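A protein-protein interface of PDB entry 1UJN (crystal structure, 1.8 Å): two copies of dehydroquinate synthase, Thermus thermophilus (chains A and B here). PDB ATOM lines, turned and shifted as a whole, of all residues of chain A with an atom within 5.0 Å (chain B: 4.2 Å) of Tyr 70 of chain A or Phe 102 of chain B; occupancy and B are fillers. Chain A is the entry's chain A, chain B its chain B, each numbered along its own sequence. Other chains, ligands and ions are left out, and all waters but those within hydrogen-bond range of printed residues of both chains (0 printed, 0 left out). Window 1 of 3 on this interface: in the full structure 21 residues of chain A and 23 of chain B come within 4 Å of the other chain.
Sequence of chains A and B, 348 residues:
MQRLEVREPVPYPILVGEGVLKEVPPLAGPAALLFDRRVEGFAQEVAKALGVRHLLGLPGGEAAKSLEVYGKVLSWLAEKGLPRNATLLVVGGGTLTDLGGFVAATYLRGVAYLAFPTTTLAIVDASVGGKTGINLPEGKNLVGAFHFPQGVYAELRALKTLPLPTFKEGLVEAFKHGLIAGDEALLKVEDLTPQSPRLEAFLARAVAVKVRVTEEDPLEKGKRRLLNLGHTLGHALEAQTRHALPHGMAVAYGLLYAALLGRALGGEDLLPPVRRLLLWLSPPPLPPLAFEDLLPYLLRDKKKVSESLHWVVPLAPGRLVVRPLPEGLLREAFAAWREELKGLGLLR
The side-chain hydroxyl of Tyr 70 of chain A lies within hydrogen-bond range of the side-chain hydroxyl of Thr 106 of chain A, at 2.7 Å.
The side-chain hydroxyl (OG1) of Thr 106 of chain A sits at hydrogen-bond distance from the backbone carbonyl oxygen (O) of Phe 102 of chain A (2.9 Å).
The side-chain hydroxyl (OH) of Tyr 70 of chain B is in hydrogen-bond range of the side-chain hydroxyl (OG1) of Thr 106 of chain B, 2.7 Å away.
N of Ile 134 of chain B sits at hydrogen-bond distance from O of Val 143 of chain B, at 2.8 Å.
O of Phe 102 of chain B sits at hydrogen-bond distance from OG1 of Thr 106 of chain B.
N of Phe 102 of chain B lies close to OG1 of Thr 132 of chain B (3.5 Å).
O of Thr 106 of chain A lies within hydrogen-bond range of N of Gly 144 of chain B (2.8 Å).
Among the printed residues, pairs that only touch across the chains: Thr 106 of chain A with Val 143 of chain B (3.4 Å), Tyr 70 of chain A with Val 143 of chain B (3.5 Å), Tyr 70 of chain A with Phe 102 of chain B (3.6 Å), Phe 102 of chain A with Tyr 70 of chain B (3.7 Å), Phe 102 of chain A with Thr 106 of chain B (3.8 Å), Leu 74 of chain A with Val 143 of chain B (3.8 Å) and Thr 106 of chain A with Phe 102 of chain B (3.8 Å).
Of the 14 printed residues of chain A, 4 touch a printed residue of chain B.
Of the 16 printed residues of chain B, 5 touch a printed residue of chain A.
Hydrophobic or aromatic side chains of chain B that line the printed part of chain A: Tyr 70, Phe 102 and Val 143.
Among the printed residues, no Asp or Glu carboxylate lies within 4 Å of a Lys or Arg side-chain nitrogen of the other chain.
Of chain B, only Phe 102 and Val 143 come within 4 Å of Tyr 70 of chain A.
Of the printed residues of chain B, Phe 102 of chain A touches Tyr 70 and Thr 106.
Phe 102 of chain B touches just these residues of chain A: Tyr 70 (3.6 Å) and Thr 106 (3.8 Å).
Of the printed residues of chain A, Thr 106 of chain B touches Phe 102.
Ile 134 of chain B touches none of the printed residues of chain A.
The nearest residue of chain B that does not touch Tyr 70 of chain A is Tyr 70 of chain B (4.1 Å).
The nearest printed residue of chain B that does not touch Leu 74 of chain A is Ile 134 of chain B (6.3 Å).
Tyr 70 of chain A touches Phe 102 of chain B, and with the chains exchanged Phe 102 of chain A touches Tyr 70 of chain B.
Phe 102 of chain A touches Thr 106 of chain B, and with the chains exchanged Thr 106 of chain A touches Phe 102 of chain B.
Positions printed for both chains: 70, 99, 102, 103, 106 and 134.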
ATOM      1  N   SER A  66     -17.145 -10.555  16.856  1.00  0.00           N
ATOM      2  CA  SER A  66     -16.520 -10.031  15.649  1.00  0.00           C
ATOM      3  C   SER A  66     -17.180 -10.589  14.397  1.00  0.00           C
ATOM      4  O   SER A  66     -17.859 -11.613  14.446  1.00  0.00           O
ATOM      5  CB  SER A  66     -15.041 -10.406  15.623  1.00  0.00           C
ATOM      6  OG  SER A  66     -14.895 -11.799  15.407  1.00  0.00           O
ATOM      7  N   LEU A  67     -16.953  -9.921  13.271  1.00  0.00           N
ATOM      8  CA  LEU A  67     -17.516 -10.352  11.996  1.00  0.00           C
ATOM      9  C   LEU A  67     -16.964 -11.714  11.603  1.00  0.00           C
ATOM     10  O   LEU A  67     -17.662 -12.531  11.006  1.00  0.00           O
ATOM     11  CB  LEU A  67     -17.193  -9.331  10.899  1.00  0.00           C
ATOM     12  CG  LEU A  67     -17.985  -8.021  10.910  1.00  0.00           C
ATOM     13  CD1 LEU A  67     -17.298  -6.982  10.028  1.00  0.00           C
ATOM     14  CD2 LEU A  67     -19.403  -8.289  10.431  1.00  0.00           C
ATOM     15  N   GLU A  68     -15.705 -11.963  11.945  1.00  0.00           N
ATOM     16  CA  GLU A  68     -15.085 -13.232  11.604  1.00  0.00           C
ATOM     17  C   GLU A  68     -15.739 -14.409  12.321  1.00  0.00           C
ATOM     18  O   GLU A  68     -16.044 -15.428  11.701  1.00  0.00           O
ATOM     19  CB  GLU A  68     -13.589 -13.204  11.933  1.00  0.00           C
ATOM     20  CG  GLU A  68     -12.869 -14.469  11.504  1.00  0.00           C
ATOM     21  CD  GLU A  68     -13.092 -14.790  10.034  1.00  0.00           C
ATOM     22  OE1 GLU A  68     -12.569 -14.045   9.175  1.00  0.00           O
ATOM     23  OE2 GLU A  68     -13.800 -15.780   9.739  1.00  0.00           O
ATOM     24  N   VAL A  69     -15.958 -14.274  13.623  1.00  0.00           N
ATOM     25  CA  VAL A  69     -16.569 -15.360  14.385  1.00  0.00           C
ATOM     26  C   VAL A  69     -18.033 -15.528  13.975  1.00  0.00           C
ATOM     27  O   VAL A  69     -18.551 -16.645  13.916  1.00  0.00           O
ATOM     28  CB  VAL A  69     -16.467 -15.093  15.898  1.00  0.00           C
ATOM     29  CG1 VAL A  69     -17.124 -16.216  16.680  1.00  0.00           C
ATOM     30  CG2 VAL A  69     -15.005 -14.975  16.294  1.00  0.00           C
ATOM     31  N   TYR A  70     -18.681 -14.406  13.682  1.00  0.00           N
ATOM     32  CA  TYR A  70     -20.076 -14.387  13.252  1.00  0.00           C
ATOM     33  C   TYR A  70     -20.211 -15.215  11.971  1.00  0.00           C
ATOM     34  O   TYR A  70     -21.075 -16.093  11.860  1.00  0.00           O
ATOM     35  CB  TYR A  70     -20.493 -12.929  13.015  1.00  0.00           C
ATOM     36  CG  TYR A  70     -21.839 -12.706  12.345  1.00  0.00           C
ATOM     37  CD1 TYR A  70     -23.034 -13.055  12.980  1.00  0.00           C
ATOM     38  CD2 TYR A  70     -21.914 -12.107  11.091  1.00  0.00           C
ATOM     39  CE1 TYR A  70     -24.274 -12.807  12.370  1.00  0.00           C
ATOM     40  CE2 TYR A  70     -23.153 -11.850  10.472  1.00  0.00           C
ATOM     41  CZ  TYR A  70     -24.321 -12.202  11.117  1.00  0.00           C
ATOM     42  OH  TYR A  70     -25.532 -11.947  10.507  1.00  0.00           O
ATOM     43  N   GLY A  71     -19.340 -14.938  11.006  1.00  0.00           N
ATOM     44  CA  GLY A  71     -19.372 -15.666   9.756  1.00  0.00           C
ATOM     45  C   GLY A  71     -19.075 -17.137   9.951  1.00  0.00           C
ATOM     46  O   GLY A  71     -19.681 -17.987   9.305  1.00  0.00           O
ATOM     47  N   LYS A  72     -18.142 -17.437  10.850  1.00  0.00           N
ATOM     48  CA  LYS A  72     -17.764 -18.820  11.130  1.00  0.00           C
ATOM     49  C   LYS A  72     -18.937 -19.610  11.695  1.00  0.00           C
ATOM     50  O   LYS A  72     -19.209 -20.725  11.257  1.00  0.00           O
ATOM     51  CB  LYS A  72     -16.597 -18.869  12.122  1.00  0.00           C
ATOM     52  CG  LYS A  72     -15.973 -20.253  12.257  1.00  0.00           C
ATOM     53  CD  LYS A  72     -14.709 -20.216  13.110  1.00  0.00           C
ATOM     54  CE  LYS A  72     -15.038 -20.169  14.590  1.00  0.00           C
ATOM     55  NZ  LYS A  72     -15.311 -21.537  15.118  1.00  0.00           N
ATOM     56  N   VAL A  73     -19.635 -19.029  12.667  1.00  0.00           N
ATOM     57  CA  VAL A  73     -20.774 -19.711  13.272  1.00  0.00           C
ATOM     58  C   VAL A  73     -21.883 -19.924  12.246  1.00  0.00           C
ATOM     59  O   VAL A  73     -22.471 -21.001  12.176  1.00  0.00           O
ATOM     60  CB  VAL A  73     -21.324 -18.922  14.486  1.00  0.00           C
ATOM     61  CG1 VAL A  73     -22.498 -19.679  15.111  1.00  0.00           C
ATOM     62  CG2 VAL A  73     -20.214 -18.724  15.520  1.00  0.00           C
ATOM     63  N   LEU A  74     -22.173 -18.906  11.443  1.00  0.00           N
ATOM     64  CA  LEU A  74     -23.213 -19.042  10.427  1.00  0.00           C
ATOM     65  C   LEU A  74     -22.897 -20.170   9.433  1.00  0.00           C
ATOM     66  O   LEU A  74     -23.763 -20.976   9.098  1.00  0.00           O
ATOM     67  CB  LEU A  74     -23.399 -17.713   9.687  1.00  0.00           C
ATOM     68  CG  LEU A  74     -24.036 -16.589  10.515  1.00  0.00           C
ATOM     69  CD1 LEU A  74     -23.811 -15.256   9.816  1.00  0.00           C
ATOM     70  CD2 LEU A  74     -25.533 -16.854  10.702  1.00  0.00           C
ATOM     71  N   LEU A  99     -23.229 -12.602  20.700  1.00  0.00           N
ATOM     72  CA  LEU A  99     -22.888 -13.207  19.416  1.00  0.00           C
ATOM     73  C   LEU A  99     -23.932 -14.237  18.986  1.00  0.00           C
ATOM     74  O   LEU A  99     -24.484 -14.151  17.886  1.00  0.00           O
ATOM     75  CB  LEU A  99     -21.519 -13.883  19.502  1.00  0.00           C
ATOM     76  CG  LEU A  99     -21.133 -14.746  18.297  1.00  0.00           C
ATOM     77  CD1 LEU A  99     -20.835 -13.850  17.102  1.00  0.00           C
ATOM     78  CD2 LEU A  99     -19.935 -15.595  18.645  1.00  0.00           C
ATOM     79  N   PHE A 102     -27.316 -12.868  17.990  1.00  0.00           N
ATOM     80  CA  PHE A 102     -27.276 -12.193  16.694  1.00  0.00           C
ATOM     81  C   PHE A 102     -27.240 -13.218  15.561  1.00  0.00           C
ATOM     82  O   PHE A 102     -27.857 -13.019  14.506  1.00  0.00           O
ATOM     83  CB  PHE A 102     -26.062 -11.261  16.629  1.00  0.00           C
ATOM     84  CG  PHE A 102     -25.984 -10.455  15.361  1.00  0.00           C
ATOM     85  CD1 PHE A 102     -27.096  -9.753  14.897  1.00  0.00           C
ATOM     86  CD2 PHE A 102     -24.798 -10.395  14.633  1.00  0.00           C
ATOM     87  CE1 PHE A 102     -27.029  -9.001  13.726  1.00  0.00           C
ATOM     88  CE2 PHE A 102     -24.715  -9.645  13.456  1.00  0.00           C
ATOM     89  CZ  PHE A 102     -25.834  -8.946  12.999  1.00  0.00           C
ATOM     90  N   VAL A 103     -26.518 -14.314  15.780  1.00  0.00           N
ATOM     91  CA  VAL A 103     -26.460 -15.386  14.793  1.00  0.00           C
ATOM     92  C   VAL A 103     -27.884 -15.937  14.639  1.00  0.00           C
ATOM     93  O   VAL A 103     -28.360 -16.129  13.529  1.00  0.00           O
ATOM     94  CB  VAL A 103     -25.509 -16.511  15.254  1.00  0.00           C
ATOM     95  CG1 VAL A 103     -25.714 -17.768  14.405  1.00  0.00           C
ATOM     96  CG2 VAL A 103     -24.057 -16.032  15.123  1.00  0.00           C
ATOM     97  N   THR A 106     -30.270 -13.713  12.642  1.00  0.00           N
ATOM     98  CA  THR A 106     -30.043 -13.573  11.214  1.00  0.00           C
ATOM     99  C   THR A 106     -29.890 -14.831  10.377  1.00  0.00           C
ATOM    100  O   THR A 106     -30.013 -14.765   9.156  1.00  0.00           O
ATOM    101  CB  THR A 106     -28.828 -12.663  10.975  1.00  0.00           C
ATOM    102  OG1 THR A 106     -27.676 -13.227  11.613  1.00  0.00           O
ATOM    103  CG2 THR A 106     -29.098 -11.262  11.561  1.00  0.00           C
ATOM    104  N   ILE A 134     -22.469  -7.574  17.629  1.00  0.00           N
ATOM    105  CA  ILE A 134     -21.026  -7.744  17.620  1.00  0.00           C
ATOM    106  C   ILE A 134     -20.345  -6.378  17.494  1.00  0.00           C
ATOM    107  O   ILE A 134     -21.016  -5.348  17.360  1.00  0.00           O
ATOM    108  CB  ILE A 134     -20.592  -8.643  16.438  1.00  0.00           C
ATOM    109  CG1 ILE A 134     -21.096  -8.048  15.119  1.00  0.00           C
ATOM    110  CG2 ILE A 134     -21.160 -10.058  16.617  1.00  0.00           C
ATOM    111  CD1 ILE A 134     -20.575  -8.755  13.878  1.00  0.00           C
ATOM    112  N   TYR B  70     -20.510  -6.883   3.165  1.00  0.00           N
ATOM    113  CA  TYR B  70     -21.375  -6.539   4.288  1.00  0.00           C
ATOM    114  C   TYR B  70     -20.520  -5.861   5.367  1.00  0.00           C
ATOM    115  O   TYR B  70     -20.857  -4.784   5.850  1.00  0.00           O
ATOM    116  CB  TYR B  70     -22.030  -7.821   4.814  1.00  0.00           C
ATOM    117  CG  TYR B  70     -22.791  -7.685   6.116  1.00  0.00           C
ATOM    118  CD1 TYR B  70     -23.971  -6.948   6.191  1.00  0.00           C
ATOM    119  CD2 TYR B  70     -22.340  -8.330   7.267  1.00  0.00           C
ATOM    120  CE1 TYR B  70     -24.693  -6.859   7.391  1.00  0.00           C
ATOM    121  CE2 TYR B  70     -23.046  -8.251   8.463  1.00  0.00           C
ATOM    122  CZ  TYR B  70     -24.220  -7.518   8.519  1.00  0.00           C
ATOM    123  OH  TYR B  70     -24.917  -7.461   9.697  1.00  0.00           O
ATOM    124  N   ASP B  98     -30.933  -6.360  -1.352  1.00  0.00           N
ATOM    125  CA  ASP B  98     -30.775  -7.510  -0.458  1.00  0.00           C
ATOM    126  C   ASP B  98     -29.664  -7.124   0.520  1.00  0.00           C
ATOM    127  O   ASP B  98     -29.830  -7.192   1.739  1.00  0.00           O
ATOM    128  CB  ASP B  98     -30.333  -8.759  -1.235  1.00  0.00           C
ATOM    129  CG  ASP B  98     -31.477  -9.437  -1.966  1.00  0.00           C
ATOM    130  OD1 ASP B  98     -31.200 -10.292  -2.846  1.00  0.00           O
ATOM    131  OD2 ASP B  98     -32.648  -9.131  -1.657  1.00  0.00           O
ATOM    132  N   LEU B  99     -28.522  -6.717  -0.029  1.00  0.00           N
ATOM    133  CA  LEU B  99     -27.388  -6.322   0.789  1.00  0.00           C
ATOM    134  C   LEU B  99     -27.687  -5.069   1.601  1.00  0.00           C
ATOM    135  O   LEU B  99     -27.503  -5.049   2.820  1.00  0.00           O
ATOM    136  CB  LEU B  99     -26.156  -6.067  -0.094  1.00  0.00           C
ATOM    137  CG  LEU B  99     -24.993  -5.337   0.595  1.00  0.00           C
ATOM    138  CD1 LEU B  99     -24.427  -6.202   1.728  1.00  0.00           C
ATOM    139  CD2 LEU B  99     -23.916  -5.024  -0.427  1.00  0.00           C
ATOM    140  N   GLY B 100     -28.147  -4.027   0.911  1.00  0.00           N
ATOM    141  CA  GLY B 100     -28.431  -2.764   1.568  1.00  0.00           C
ATOM    142  C   GLY B 100     -29.489  -2.841   2.650  1.00  0.00           C
ATOM    143  O   GLY B 100     -29.357  -2.203   3.699  1.00  0.00           O
ATOM    144  N   GLY B 101     -30.543  -3.612   2.398  1.00  0.00           N
ATOM    145  CA  GLY B 101     -31.600  -3.736   3.383  1.00  0.00           C
ATOM    146  C   GLY B 101     -31.113  -4.505   4.596  1.00  0.00           C
ATOM    147  O   GLY B 101     -31.564  -4.265   5.716  1.00  0.00           O
ATOM    148  N   PHE B 102     -30.184  -5.435   4.386  1.00  0.00           N
ATOM    149  CA  PHE B 102     -29.670  -6.217   5.505  1.00  0.00           C
ATOM    150  C   PHE B 102     -28.706  -5.368   6.331  1.00  0.00           C
ATOM    151  O   PHE B 102     -28.635  -5.503   7.555  1.00  0.00           O
ATOM    152  CB  PHE B 102     -28.988  -7.495   5.005  1.00  0.00           C
ATOM    153  CG  PHE B 102     -28.470  -8.376   6.112  1.00  0.00           C
ATOM    154  CD1 PHE B 102     -29.316  -8.792   7.139  1.00  0.00           C
ATOM    155  CD2 PHE B 102     -27.139  -8.786   6.130  1.00  0.00           C
ATOM    156  CE1 PHE B 102     -28.846  -9.606   8.173  1.00  0.00           C
ATOM    157  CE2 PHE B 102     -26.657  -9.598   7.155  1.00  0.00           C
ATOM    158  CZ  PHE B 102     -27.518 -10.010   8.185  1.00  0.00           C
ATOM    159  N   VAL B 103     -27.957  -4.497   5.663  1.00  0.00           N
ATOM    160  CA  VAL B 103     -27.046  -3.601   6.361  1.00  0.00           C
ATOM    161  C   VAL B 103     -27.915  -2.660   7.207  1.00  0.00           C
ATOM    162  O   VAL B 103     -27.643  -2.436   8.388  1.00  0.00           O
ATOM    163  CB  VAL B 103     -26.209  -2.758   5.371  1.00  0.00           C
ATOM    164  CG1 VAL B 103     -25.559  -1.589   6.103  1.00  0.00           C
ATOM    165  CG2 VAL B 103     -25.143  -3.635   4.718  1.00  0.00           C
ATOM    166  N   ALA B 104     -28.958  -2.112   6.592  1.00  0.00           N
ATOM    167  CA  ALA B 104     -29.866  -1.209   7.297  1.00  0.00           C
ATOM    168  C   ALA B 104     -30.546  -1.922   8.468  1.00  0.00           C
ATOM    169  O   ALA B 104     -30.796  -1.324   9.505  1.00  0.00           O
ATOM    170  CB  ALA B 104     -30.926  -0.671   6.342  1.00  0.00           C
ATOM    171  N   ALA B 105     -30.844  -3.202   8.297  1.00  0.00           N
ATOM    172  CA  ALA B 105     -31.506  -3.960   9.354  1.00  0.00           C
ATOM    173  C   ALA B 105     -30.625  -4.217  10.574  1.00  0.00           C
ATOM    174  O   ALA B 105     -31.132  -4.383  11.687  1.00  0.00           O
ATOM    175  CB  ALA B 105     -32.009  -5.298   8.795  1.00  0.00           C
ATOM    176  N   THR B 106     -29.311  -4.223  10.377  1.00  0.00           N
ATOM    177  CA  THR B 106     -28.399  -4.545  11.464  1.00  0.00           C
ATOM    178  C   THR B 106     -27.460  -3.450  11.940  1.00  0.00           C
ATOM    179  O   THR B 106     -26.902  -3.553  13.027  1.00  0.00           O
ATOM    180  CB  THR B 106     -27.571  -5.786  11.091  1.00  0.00           C
ATOM    181  OG1 THR B 106     -26.866  -5.538   9.866  1.00  0.00           O
ATOM    182  CG2 THR B 106     -28.495  -6.995  10.906  1.00  0.00           C
ATOM    183  N   THR B 132     -34.396  -9.331   3.016  1.00  0.00           N
ATOM    184  CA  THR B 132     -33.043  -8.804   2.830  1.00  0.00           C
ATOM    185  C   THR B 132     -32.073  -9.897   3.241  1.00  0.00           C
ATOM    186  O   THR B 132     -32.457 -10.845   3.933  1.00  0.00           O
ATOM    187  CB  THR B 132     -32.753  -7.542   3.695  1.00  0.00           C
ATOM    188  OG1 THR B 132     -32.552  -7.919   5.066  1.00  0.00           O
ATOM    189  CG2 THR B 132     -33.914  -6.560   3.617  1.00  0.00           C
ATOM    190  N   GLY B 133     -30.820  -9.785   2.805  1.00  0.00           N
ATOM    191  CA  GLY B 133     -29.858 -10.797   3.189  1.00  0.00           C
ATOM    192  C   GLY B 133     -28.652 -10.912   2.288  1.00  0.00           C
ATOM    193  O   GLY B 133     -28.531 -10.202   1.280  1.00  0.00           O
ATOM    194  N   ILE B 134     -27.768 -11.833   2.654  1.00  0.00           N
ATOM    195  CA  ILE B 134     -26.535 -12.071   1.913  1.00  0.00           C
ATOM    196  C   ILE B 134     -26.272 -13.563   1.739  1.00  0.00           C
ATOM    197  O   ILE B 134     -27.057 -14.405   2.197  1.00  0.00           O
ATOM    198  CB  ILE B 134     -25.330 -11.419   2.626  1.00  0.00           C
ATOM    199  CG1 ILE B 134     -25.195 -11.965   4.049  1.00  0.00           C
ATOM    200  CG2 ILE B 134     -25.500  -9.898   2.651  1.00  0.00           C
ATOM    201  CD1 ILE B 134     -23.991 -11.424   4.790  1.00  0.00           C
ATOM    202  N   VAL B 143     -28.387 -15.943   5.163  1.00  0.00           N
ATOM    203  CA  VAL B 143     -28.268 -14.998   6.272  1.00  0.00           C
ATOM    204  C   VAL B 143     -29.065 -13.756   5.905  1.00  0.00           C
ATOM    205  O   VAL B 143     -28.989 -13.292   4.774  1.00  0.00           O
ATOM    206  CB  VAL B 143     -26.796 -14.578   6.500  1.00  0.00           C
ATOM    207  CG1 VAL B 143     -26.707 -13.611   7.684  1.00  0.00           C
ATOM    208  CG2 VAL B 143     -25.930 -15.802   6.749  1.00  0.00           C
ATOM    209  N   GLY B 144     -29.837 -13.210   6.836  1.00  0.00           N
ATOM    210  CA  GLY B 144     -30.587 -12.017   6.481  1.00  0.00           C
ATOM    211  C   GLY B 144     -31.562 -11.547   7.533  1.00  0.00           C
ATOM    212  O   GLY B 144     -31.423 -11.877   8.703  1.00  0.00           O
ATOM    213  N   ALA B 145     -32.550 -10.772   7.109  1.00  0.00           N
ATOM    214  CA  ALA B 145     -33.550 -10.256   8.031  1.00  0.00           C
ATOM    215  C   ALA B 145     -34.749  -9.731   7.280  1.00  0.00           C
ATOM    216  O   ALA B 145     -34.658  -9.363   6.108  1.00  0.00           O
ATOM    217  CB  ALA B 145     -32.952  -9.129   8.869  1.00  0.00           C
